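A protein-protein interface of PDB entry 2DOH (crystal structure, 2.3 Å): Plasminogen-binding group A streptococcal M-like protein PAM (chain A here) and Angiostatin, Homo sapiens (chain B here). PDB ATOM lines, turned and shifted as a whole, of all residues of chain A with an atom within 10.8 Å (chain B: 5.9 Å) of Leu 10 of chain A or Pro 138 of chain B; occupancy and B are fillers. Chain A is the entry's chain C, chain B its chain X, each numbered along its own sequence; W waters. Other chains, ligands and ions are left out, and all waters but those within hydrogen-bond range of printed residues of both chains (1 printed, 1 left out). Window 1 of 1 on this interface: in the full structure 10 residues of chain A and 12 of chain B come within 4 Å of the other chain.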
ATOM      1  N   LEU A   4      19.582   8.323  21.225  1.00  0.00           N
ATOM      2  CA  LEU A   4      19.434   9.247  20.056  1.00  0.00           C
ATOM      3  C   LEU A   4      19.004   8.487  18.793  1.00  0.00           C
ATOM      4  O   LEU A   4      19.609   8.626  17.726  1.00  0.00           O
ATOM      5  CB  LEU A   4      20.755   9.997  19.811  1.00  0.00           C
ATOM      6  CG  LEU A   4      20.923  11.365  20.481  1.00  0.00           C
ATOM      7  CD1 LEU A   4      22.347  11.865  20.303  1.00  0.00           C
ATOM      8  CD2 LEU A   4      19.919  12.383  19.925  1.00  0.00           C
ATOM      9  N   THR A   5      17.952   7.685  18.919  1.00  0.00           N
ATOM     10  CA  THR A   5      17.444   6.924  17.784  1.00  0.00           C
ATOM     11  C   THR A   5      16.700   7.832  16.817  1.00  0.00           C
ATOM     12  O   THR A   5      16.391   8.999  17.109  1.00  0.00           O
ATOM     13  CB  THR A   5      16.500   5.785  18.235  1.00  0.00           C
ATOM     14  OG1 THR A   5      15.439   6.319  19.039  1.00  0.00           O
ATOM     15  CG2 THR A   5      17.210   4.793  19.156  1.00  0.00           C
ATOM     16  N   ALA A   6      16.416   7.259  15.655  1.00  0.00           N
ATOM     17  CA  ALA A   6      15.682   7.940  14.620  1.00  0.00           C
ATOM     18  C   ALA A   6      14.300   8.258  15.149  1.00  0.00           C
ATOM     19  O   ALA A   6      13.780   9.337  14.949  1.00  0.00           O
ATOM     20  CB  ALA A   6      15.593   7.051  13.387  1.00  0.00           C
ATOM     21  N   ASP A   7      13.709   7.296  15.835  1.00  0.00           N
ATOM     22  CA  ASP A   7      12.335   7.443  16.247  1.00  0.00           C
ATOM     23  C   ASP A   7      12.196   8.440  17.371  1.00  0.00           C
ATOM     24  O   ASP A   7      11.147   9.056  17.512  1.00  0.00           O
ATOM     25  CB  ASP A   7      11.740   6.089  16.619  1.00  0.00           C
ATOM     26  CG  ASP A   7      11.217   5.365  15.405  1.00  0.00           C
ATOM     27  OD1 ASP A   7      11.932   4.487  14.881  1.00  0.00           O
ATOM     28  OD2 ASP A   7      10.116   5.643  14.876  1.00  0.00           O
ATOM     29  N   ALA A   8      13.248   8.585  18.175  1.00  0.00           N
ATOM     30  CA  ALA A   8      13.254   9.607  19.217  1.00  0.00           C
ATOM     31  C   ALA A   8      13.312  10.985  18.568  1.00  0.00           C
ATOM     32  O   ALA A   8      12.673  11.908  19.038  1.00  0.00           O
ATOM     33  CB  ALA A   8      14.420   9.429  20.159  1.00  0.00           C
ATOM     34  N   GLU A   9      14.101  11.126  17.509  1.00  0.00           N
ATOM     35  CA  GLU A   9      14.189  12.394  16.810  1.00  0.00           C
ATOM     36  C   GLU A   9      12.849  12.725  16.158  1.00  0.00           C
ATOM     37  O   GLU A   9      12.346  13.823  16.279  1.00  0.00           O
ATOM     38  CB  GLU A   9      15.301  12.389  15.754  1.00  0.00           C
ATOM     39  CG  GLU A   9      16.292  13.520  15.944  1.00  0.00           C
ATOM     40  CD  GLU A   9      16.709  14.239  14.671  1.00  0.00           C
ATOM     41  OE1 GLU A   9      17.468  13.640  13.872  1.00  0.00           O
ATOM     42  OE2 GLU A   9      16.323  15.422  14.504  1.00  0.00           O
ATOM     43  N   LEU A  10      12.262  11.763  15.473  1.00  0.00           N
ATOM     44  CA  LEU A  10      10.979  12.015  14.829  1.00  0.00           C
ATOM     45  C   LEU A  10       9.929  12.457  15.821  1.00  0.00           C
ATOM     46  O   LEU A  10       9.035  13.205  15.467  1.00  0.00           O
ATOM     47  CB  LEU A  10      10.493  10.782  14.082  1.00  0.00           C
ATOM     48  CG  LEU A  10      11.351  10.552  12.871  1.00  0.00           C
ATOM     49  CD1 LEU A  10      11.224   9.087  12.402  1.00  0.00           C
ATOM     50  CD2 LEU A  10      10.976  11.538  11.793  1.00  0.00           C
ATOM     51  N   GLN A  11      10.040  11.995  17.061  1.00  0.00           N
ATOM     52  CA  GLN A  11       9.044  12.299  18.073  1.00  0.00           C
ATOM     53  C   GLN A  11       9.212  13.727  18.595  1.00  0.00           C
ATOM     54  O   GLN A  11       8.228  14.433  18.847  1.00  0.00           O
ATOM     55  CB  GLN A  11       9.139  11.267  19.205  1.00  0.00           C
ATOM     56  CG  GLN A  11       8.400  11.629  20.499  1.00  0.00           C
ATOM     57  CD  GLN A  11       6.932  11.292  20.445  1.00  0.00           C
ATOM     58  OE1 GLN A  11       6.533  10.211  20.849  1.00  0.00           O
ATOM     59  NE2 GLN A  11       6.124  12.224  19.952  1.00  0.00           N
ATOM     60  N   ARG A  12      10.459  14.150  18.759  1.00  0.00           N
ATOM     61  CA  ARG A  12      10.752  15.536  19.131  1.00  0.00           C
ATOM     62  C   ARG A  12      10.316  16.443  18.017  1.00  0.00           C
ATOM     63  O   ARG A  12       9.759  17.495  18.288  1.00  0.00           O
ATOM     64  CB  ARG A  12      12.229  15.760  19.402  1.00  0.00           C
ATOM     65  CG  ARG A  12      12.677  15.077  20.623  1.00  0.00           C
ATOM     66  CD  ARG A  12      14.066  15.468  21.038  1.00  0.00           C
ATOM     67  NE  ARG A  12      14.940  15.523  19.876  1.00  0.00           N
ATOM     68  CZ  ARG A  12      15.786  14.561  19.555  1.00  0.00           C
ATOM     69  NH1 ARG A  12      15.907  13.471  20.324  1.00  0.00           N
ATOM     70  NH2 ARG A  12      16.548  14.703  18.476  1.00  0.00           N
ATOM     71  N   LEU A  13      10.579  16.025  16.779  1.00  0.00           N
ATOM     72  CA  LEU A  13      10.171  16.779  15.615  1.00  0.00           C
ATOM     73  C   LEU A  13       8.641  16.981  15.597  1.00  0.00           C
ATOM     74  O   LEU A  13       8.180  18.080  15.324  1.00  0.00           O
ATOM     75  CB  LEU A  13      10.660  16.128  14.319  1.00  0.00           C
ATOM     76  CG  LEU A  13      12.165  16.272  14.060  1.00  0.00           C
ATOM     77  CD1 LEU A  13      12.614  15.369  12.914  1.00  0.00           C
ATOM     78  CD2 LEU A  13      12.560  17.727  13.768  1.00  0.00           C
ATOM     79  N   LYS A  14       7.869  15.936  15.886  1.00  0.00           N
ATOM     80  CA  LYS A  14       6.415  16.072  15.855  1.00  0.00           C
ATOM     81  C   LYS A  14       5.991  16.999  16.987  1.00  0.00           C
ATOM     82  O   LYS A  14       5.201  17.883  16.783  1.00  0.00           O
ATOM     83  CB  LYS A  14       5.702  14.731  15.986  1.00  0.00           C
ATOM     84  CG  LYS A  14       4.204  14.866  16.185  1.00  0.00           C
ATOM     85  CD  LYS A  14       3.503  13.540  16.049  1.00  0.00           C
ATOM     86  CE  LYS A  14       3.739  12.637  17.258  1.00  0.00           C
ATOM     87  NZ  LYS A  14       4.145  11.267  16.840  1.00  0.00           N
ATOM     88  N   ASN A  15       6.529  16.764  18.176  1.00  0.00           N
ATOM     89  CA  ASN A  15       6.251  17.592  19.342  1.00  0.00           C
ATOM     90  C   ASN A  15       6.493  19.084  19.056  1.00  0.00           C
ATOM     91  O   ASN A  15       5.740  19.934  19.495  1.00  0.00           O
ATOM     92  CB  ASN A  15       7.139  17.150  20.520  1.00  0.00           C
ATOM     93  CG  ASN A  15       6.692  15.842  21.168  1.00  0.00           C
ATOM     94  OD1 ASN A  15       5.543  15.423  21.041  1.00  0.00           O
ATOM     95  ND2 ASN A  15       7.617  15.199  21.900  1.00  0.00           N
ATOM     96  N   GLU A  16       7.558  19.393  18.331  1.00  0.00           N
ATOM     97  CA  GLU A  16       7.884  20.768  17.974  1.00  0.00           C
ATOM     98  C   GLU A  16       6.890  21.337  16.964  1.00  0.00           C
ATOM     99  O   GLU A  16       6.542  22.503  17.032  1.00  0.00           O
ATOM    100  CB  GLU A  16       9.295  20.863  17.402  1.00  0.00           C
ATOM    101  CG  GLU A  16       9.778  22.309  17.225  1.00  0.00           C
ATOM    102  CD  GLU A  16      11.215  22.418  16.706  1.00  0.00           C
ATOM    103  OE1 GLU A  16      11.641  23.532  16.386  1.00  0.00           O
ATOM    104  OE2 GLU A  16      11.925  21.404  16.619  1.00  0.00           O
ATOM    105  N   ARG A  17       6.496  20.511  16.042  1.00  0.00           N
ATOM    106  CA  ARG A  17       5.545  20.926  15.020  1.00  0.00           C
ATOM    107  C   ARG A  17       4.194  21.288  15.708  1.00  0.00           C
ATOM    108  O   ARG A  17       3.578  22.324  15.425  1.00  0.00           O
ATOM    109  CB  ARG A  17       5.317  19.801  14.014  1.00  0.00           C
ATOM    110  CG  ARG A  17       6.516  19.452  13.081  1.00  0.00           C
ATOM    111  CD  ARG A  17       6.049  18.377  12.137  1.00  0.00           C
ATOM    112  NE  ARG A  17       4.613  18.337  12.296  1.00  0.00           N
ATOM    113  CZ  ARG A  17       3.907  17.361  12.848  1.00  0.00           C
ATOM    114  NH1 ARG A  17       4.478  16.222  13.270  1.00  0.00           N
ATOM    115  NH2 ARG A  17       2.599  17.465  13.065  1.00  0.00           N
ATOM    116  N   HIS A  18       3.765  20.386  16.676  1.00  0.00           N
ATOM    117  CA  HIS A  18       2.505  20.600  17.390  1.00  0.00           C
ATOM    118  C   HIS A  18       2.574  21.872  18.264  1.00  0.00           C
ATOM    119  O   HIS A  18       1.700  22.714  18.224  1.00  0.00           O
ATOM    120  CB  HIS A  18       2.169  19.390  18.260  1.00  0.00           C
ATOM    121  CG  HIS A  18       1.658  18.212  17.490  1.00  0.00           C
ATOM    122  ND1 HIS A  18       1.864  18.062  16.140  1.00  0.00           N
ATOM    123  CD2 HIS A  18       0.953  17.126  17.882  1.00  0.00           C
ATOM    124  CE1 HIS A  18       1.299  16.943  15.731  1.00  0.00           C
ATOM    125  NE2 HIS A  18       0.739  16.355  16.770  1.00  0.00           N
ATOM    126  N   GLU B  92       0.915   5.264   8.266  1.00  0.00           N
ATOM    127  CA  GLU B  92       2.291   5.016   8.672  1.00  0.00           C
ATOM    128  C   GLU B  92       3.122   4.527   7.483  1.00  0.00           C
ATOM    129  O   GLU B  92       4.246   4.978   7.282  1.00  0.00           O
ATOM    130  CB  GLU B  92       2.308   4.004   9.815  1.00  0.00           C
ATOM    131  CG  GLU B  92       1.093   4.127  10.737  1.00  0.00           C
ATOM    132  CD  GLU B  92      -0.175   3.398  10.251  1.00  0.00           C
ATOM    133  OE1 GLU B  92      -0.171   2.695   9.207  1.00  0.00           O
ATOM    134  OE2 GLU B  92      -1.210   3.527  10.940  1.00  0.00           O
ATOM    135  N   TRP B 110      10.148  17.620   0.590  1.00  0.00           N
ATOM    136  CA  TRP B 110      10.902  17.221   1.779  1.00  0.00           C
ATOM    137  C   TRP B 110      12.376  17.628   1.730  1.00  0.00           C
ATOM    138  O   TRP B 110      12.982  17.956   2.762  1.00  0.00           O
ATOM    139  CB  TRP B 110      10.762  15.714   2.015  1.00  0.00           C
ATOM    140  CG  TRP B 110       9.363  15.329   2.299  1.00  0.00           C
ATOM    141  CD1 TRP B 110       8.462  14.774   1.414  1.00  0.00           C
ATOM    142  CD2 TRP B 110       8.662  15.463   3.546  1.00  0.00           C
ATOM    143  NE1 TRP B 110       7.257  14.571   2.038  1.00  0.00           N
ATOM    144  CE2 TRP B 110       7.344  14.991   3.339  1.00  0.00           C
ATOM    145  CE3 TRP B 110       9.004  15.967   4.798  1.00  0.00           C
ATOM    146  CZ2 TRP B 110       6.390  14.987   4.338  1.00  0.00           C
ATOM    147  CZ3 TRP B 110       8.055  15.963   5.799  1.00  0.00           C
ATOM    148  CH2 TRP B 110       6.766  15.470   5.572  1.00  0.00           C
ATOM    149  N   TYR B 120      13.103  17.361   8.765  1.00  0.00           N
ATOM    150  CA  TYR B 120      12.673  16.101   8.193  1.00  0.00           C
ATOM    151  C   TYR B 120      13.453  15.875   6.912  1.00  0.00           C
ATOM    152  O   TYR B 120      12.917  15.888   5.811  1.00  0.00           O
ATOM    153  CB  TYR B 120      11.184  16.097   7.965  1.00  0.00           C
ATOM    154  CG  TYR B 120      10.316  16.052   9.232  1.00  0.00           C
ATOM    155  CD1 TYR B 120      10.041  17.211   9.978  1.00  0.00           C
ATOM    156  CD2 TYR B 120       9.749  14.865   9.659  1.00  0.00           C
ATOM    157  CE1 TYR B 120       9.240  17.170  11.112  1.00  0.00           C
ATOM    158  CE2 TYR B 120       8.953  14.810  10.789  1.00  0.00           C
ATOM    159  CZ  TYR B 120       8.674  15.974  11.501  1.00  0.00           C
ATOM    160  OH  TYR B 120       7.885  15.898  12.625  1.00  0.00           O
ATOM    161  N   PHE B 125      16.298  10.232   7.226  1.00  0.00           N
ATOM    162  CA  PHE B 125      15.262   9.209   7.437  1.00  0.00           C
ATOM    163  C   PHE B 125      14.905   8.497   6.131  1.00  0.00           C
ATOM    164  O   PHE B 125      13.771   8.539   5.707  1.00  0.00           O
ATOM    165  CB  PHE B 125      13.990   9.845   8.053  1.00  0.00           C
ATOM    166  CG  PHE B 125      14.267  10.692   9.265  1.00  0.00           C
ATOM    167  CD1 PHE B 125      14.331  12.064   9.168  1.00  0.00           C
ATOM    168  CD2 PHE B 125      14.505  10.107  10.488  1.00  0.00           C
ATOM    169  CE1 PHE B 125      14.611  12.836  10.271  1.00  0.00           C
ATOM    170  CE2 PHE B 125      14.806  10.879  11.599  1.00  0.00           C
ATOM    171  CZ  PHE B 125      14.857  12.234  11.492  1.00  0.00           C
ATOM    172  N   LYS B 128      11.848   6.382   5.652  1.00  0.00           N
ATOM    173  CA  LYS B 128      10.523   7.027   5.702  1.00  0.00           C
ATOM    174  C   LYS B 128      10.059   7.556   4.339  1.00  0.00           C
ATOM    175  O   LYS B 128       8.941   8.056   4.193  1.00  0.00           O
ATOM    176  CB  LYS B 128      10.486   8.147   6.756  1.00  0.00           C
ATOM    177  CG  LYS B 128      10.739   7.680   8.216  1.00  0.00           C
ATOM    178  CD  LYS B 128       9.743   6.593   8.661  1.00  0.00           C
ATOM    179  CE  LYS B 128      10.020   6.081  10.080  1.00  0.00           C
ATOM    180  NZ  LYS B 128       8.882   5.254  10.597  1.00  0.00           N
ATOM    181  N   LEU B 130      10.574  10.040   2.300  1.00  0.00           N
ATOM    182  CA  LEU B 130      10.161  11.436   2.163  1.00  0.00           C
ATOM    183  C   LEU B 130      10.515  11.892   0.750  1.00  0.00           C
ATOM    184  O   LEU B 130      11.519  12.566   0.480  1.00  0.00           O
ATOM    185  CB  LEU B 130      10.832  12.289   3.246  1.00  0.00           C
ATOM    186  CG  LEU B 130      10.518  11.783   4.656  1.00  0.00           C
ATOM    187  CD1 LEU B 130      11.440  12.410   5.654  1.00  0.00           C
ATOM    188  CD2 LEU B 130       9.077  12.077   5.030  1.00  0.00           C
ATOM    189  N   ARG B 136       3.203  12.495   3.870  1.00  0.00           N
ATOM    190  CA  ARG B 136       3.757  11.319   4.498  1.00  0.00           C
ATOM    191  C   ARG B 136       3.494  11.326   5.981  1.00  0.00           C
ATOM    192  O   ARG B 136       3.160  12.362   6.547  1.00  0.00           O
ATOM    193  CB  ARG B 136       5.239  11.255   4.231  1.00  0.00           C
ATOM    194  CG  ARG B 136       5.561  10.962   2.794  1.00  0.00           C
ATOM    195  CD  ARG B 136       5.498   9.452   2.475  1.00  0.00           C
ATOM    196  NE  ARG B 136       5.867   9.088   1.109  1.00  0.00           N
ATOM    197  CZ  ARG B 136       5.012   9.006   0.092  1.00  0.00           C
ATOM    198  NH1 ARG B 136       3.709   9.289   0.244  1.00  0.00           N
ATOM    199  NH2 ARG B 136       5.462   8.630  -1.099  1.00  0.00           N
ATOM    200  N   ASN B 137       3.605  10.155   6.608  1.00  0.00           N
ATOM    201  CA  ASN B 137       3.469  10.060   8.051  1.00  0.00           C
ATOM    202  C   ASN B 137       4.657   9.344   8.667  1.00  0.00           C
ATOM    203  O   ASN B 137       4.567   8.170   9.054  1.00  0.00           O
ATOM    204  CB  ASN B 137       2.178   9.379   8.478  1.00  0.00           C
ATOM    205  CG  ASN B 137       1.932   9.535   9.965  1.00  0.00           C
ATOM    206  OD1 ASN B 137       2.817   9.966  10.680  1.00  0.00           O
ATOM    207  ND2 ASN B 137       0.744   9.176  10.433  1.00  0.00           N
ATOM    208  N   PRO B 138       5.772  10.068   8.739  1.00  0.00           N
ATOM    209  CA  PRO B 138       7.032   9.505   9.204  1.00  0.00           C
ATOM    210  C   PRO B 138       7.117   9.385  10.708  1.00  0.00           C
ATOM    211  O   PRO B 138       8.005   8.683  11.155  1.00  0.00           O
ATOM    212  CB  PRO B 138       8.059  10.528   8.710  1.00  0.00           C
ATOM    213  CG  PRO B 138       7.335  11.807   8.693  1.00  0.00           C
ATOM    214  CD  PRO B 138       5.926  11.478   8.338  1.00  0.00           C
ATOM    215  N   ASP B 139       6.188  10.002  11.438  1.00  0.00           N
ATOM    216  CA  ASP B 139       6.373  10.283  12.864  1.00  0.00           C
ATOM    217  C   ASP B 139       5.101  10.138  13.677  1.00  0.00           C
ATOM    218  O   ASP B 139       4.938  10.819  14.692  1.00  0.00           O
ATOM    219  CB  ASP B 139       6.878  11.714  13.040  1.00  0.00           C
ATOM    220  CG  ASP B 139       5.906  12.740  12.479  1.00  0.00           C
ATOM    221  OD1 ASP B 139       4.809  12.337  12.000  1.00  0.00           O
ATOM    222  OD2 ASP B 139       6.162  13.963  12.502  1.00  0.00           O
ATOM    223  N   ARG B 140       4.196   9.269  13.226  1.00  0.00           N
ATOM    224  CA  ARG B 140       3.042   8.889  14.020  1.00  0.00           C
ATOM    225  C   ARG B 140       2.080  10.034  14.243  1.00  0.00           C
ATOM    226  O   ARG B 140       1.490  10.171  15.318  1.00  0.00           O
ATOM    227  CB  ARG B 140       3.500   8.337  15.370  1.00  0.00           C
ATOM    228  CG  ARG B 140       3.455   6.839  15.457  1.00  0.00           C
ATOM    229  CD  ARG B 140       4.800   6.182  15.679  1.00  0.00           C
ATOM    230  NE  ARG B 140       5.482   6.655  16.888  1.00  0.00           N
ATOM    231  CZ  ARG B 140       6.581   6.083  17.377  1.00  0.00           C
ATOM    232  NH1 ARG B 140       7.090   5.017  16.754  1.00  0.00           N
ATOM    233  NH2 ARG B 140       7.176   6.557  18.484  1.00  0.00           N
ATOM    234  N   TRP B 145       0.893  14.141   6.297  1.00  0.00           N
ATOM    235  CA  TRP B 145       0.883  15.581   6.343  1.00  0.00           C
ATOM    236  C   TRP B 145       2.055  16.012   5.512  1.00  0.00           C
ATOM    237  O   TRP B 145       2.817  15.171   5.033  1.00  0.00           O
ATOM    238  CB  TRP B 145       1.039  16.095   7.777  1.00  0.00           C
ATOM    239  CG  TRP B 145       2.254  15.541   8.456  1.00  0.00           C
ATOM    240  CD1 TRP B 145       2.353  14.353   9.085  1.00  0.00           C
ATOM    241  CD2 TRP B 145       3.542  16.141   8.533  1.00  0.00           C
ATOM    242  NE1 TRP B 145       3.627  14.169   9.547  1.00  0.00           N
ATOM    243  CE2 TRP B 145       4.371  15.270   9.232  1.00  0.00           C
ATOM    244  CE3 TRP B 145       4.073  17.344   8.093  1.00  0.00           C
ATOM    245  CZ2 TRP B 145       5.710  15.550   9.480  1.00  0.00           C
ATOM    246  CZ3 TRP B 145       5.400  17.622   8.343  1.00  0.00           C
ATOM    247  CH2 TRP B 145       6.199  16.739   9.011  1.00  0.00           C
HETATM  248  O   HOH W   1       7.067   9.963  16.833  1.00  0.00           O
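O of Arg 140 of chain B is in hydrogen-bond range of NZ of Lys 14 of chain A (3.3 Å). The side-chain carboxylate (OD2) of Asp 139 of chain B is in salt-bridge range of the guanidinium group (NH1) of Arg 17 of chain A (2.9 Å). OH of Tyr 120 of chain B sits at hydrogen-bond distance from N of Lys 14 of chain A (3.3 Å). The backbone carbonyl oxygen of Leu 13 of chain A sits close to the side-chain hydroxyl of Tyr 120 of chain B, 3.5 Å away. NH1 of Arg 140 of chain B is in salt-bridge range of OD2 of Asp 7 of chain A (3.6 Å). The side-chain hydroxyl (OH) of Tyr 120 of chain B lies close to the guanidinium group (NH1) of Arg 17 of chain A. NZ of Lys 14 of chain A lies close to O of Asp 139 of chain B, 2.3 Å away.
OD1 of Asp 139 of chain B lies within hydrogen-bond range of NE1 of Trp 145 of chain B, 3.3 Å away. The side-chain carboxylate (OD2) of Asp 139 of chain B is in hydrogen-bond range of the side-chain hydroxyl (OH) of Tyr 120 of chain B (2.6 Å). NH2 of Arg 17 of chain A sits close to ND1 of His 18 of chain A, at 3.2 Å. The backbone carbonyl oxygen (O) of Arg 136 of chain B sits at hydrogen-bond distance from the backbone NH (N) of Trp 145 of chain B (2.9 Å). The side-chain amide oxygen of Asn 137 of chain B sits at hydrogen-bond distance from the backbone NH of Arg 140 of chain B (3.0 Å). OD1 of Asn 137 of chain B sits close to OD1 of Asp 139 of chain B.
Among the printed residues, merely in contact across the chains: Leu 10 of chain A with Pro 138 of chain B (3.5 Å), Arg 17 of chain A with Trp 145 of chain B (3.5 Å), Leu 10 of chain A with Asp 139 of chain B (3.6 Å), Leu 10 of chain A with Phe 125 of chain B (3.7 Å), Glu 9 of chain A with Phe 125 of chain B (3.8 Å), Ala 6 of chain A with Phe 125 of chain B (3.8 Å), Leu 10 of chain A with Tyr 120 of chain B (3.98 Å) and Leu 10 of chain A with Lys 128 of chain B (3.98 Å).
Leu 4 of chain A touches none of the printed residues of chain B. Of the printed residues of chain B, Ala 6 of chain A touches Phe 125 (3.8 Å). Of the printed residues of chain B, Asp 7 of chain A touches Arg 140 (3.6 Å). Gln 11 of chain A touches none of the printed residues of chain B. Printed residues of chain B within 4 Å of Lys 14 of chain A: Tyr 120 (3.3 Å), Asp 139 (2.3 Å) and Arg 140 (3.3 Å). Of the printed residues of chain A, Lys 128 of chain B touches Leu 10. No residue of chain A comes within 4 Å of Asn 137 of chain B. Of the printed residues of chain A, Pro 138 of chain B touches Leu 10. Printed residues of chain A within 4 Å of Asp 139 of chain B: Leu 10, Lys 14 and Arg 17.
Hydrophobic or aromatic side chains of chain B within 4 Å of the printed part of chain A: Tyr 120, Phe 125 and Trp 145. Of the 15 printed residues of chain A, 7 touch a printed residue of chain B. Printed residues of chain A that touch a printed residue of chain B: Ala 6, Asp 7, Glu 9, Leu 10, Leu 13, Lys 14 and Arg 17. Among the printed residues, 15 pairs touch across the chains. Among the printed residues, Asp or Glu carboxylates within 4 Å of a Lys or Arg side-chain nitrogen of the other chain: Asp 7 of chain A with Arg 140 of chain B and Arg 17 of chain A with Asp 139 of chain B.
Water W1 bridges O of Asp 139 of chain B (3.1 Å) and NZ of Lys 14 of chain A (3.2 Å).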
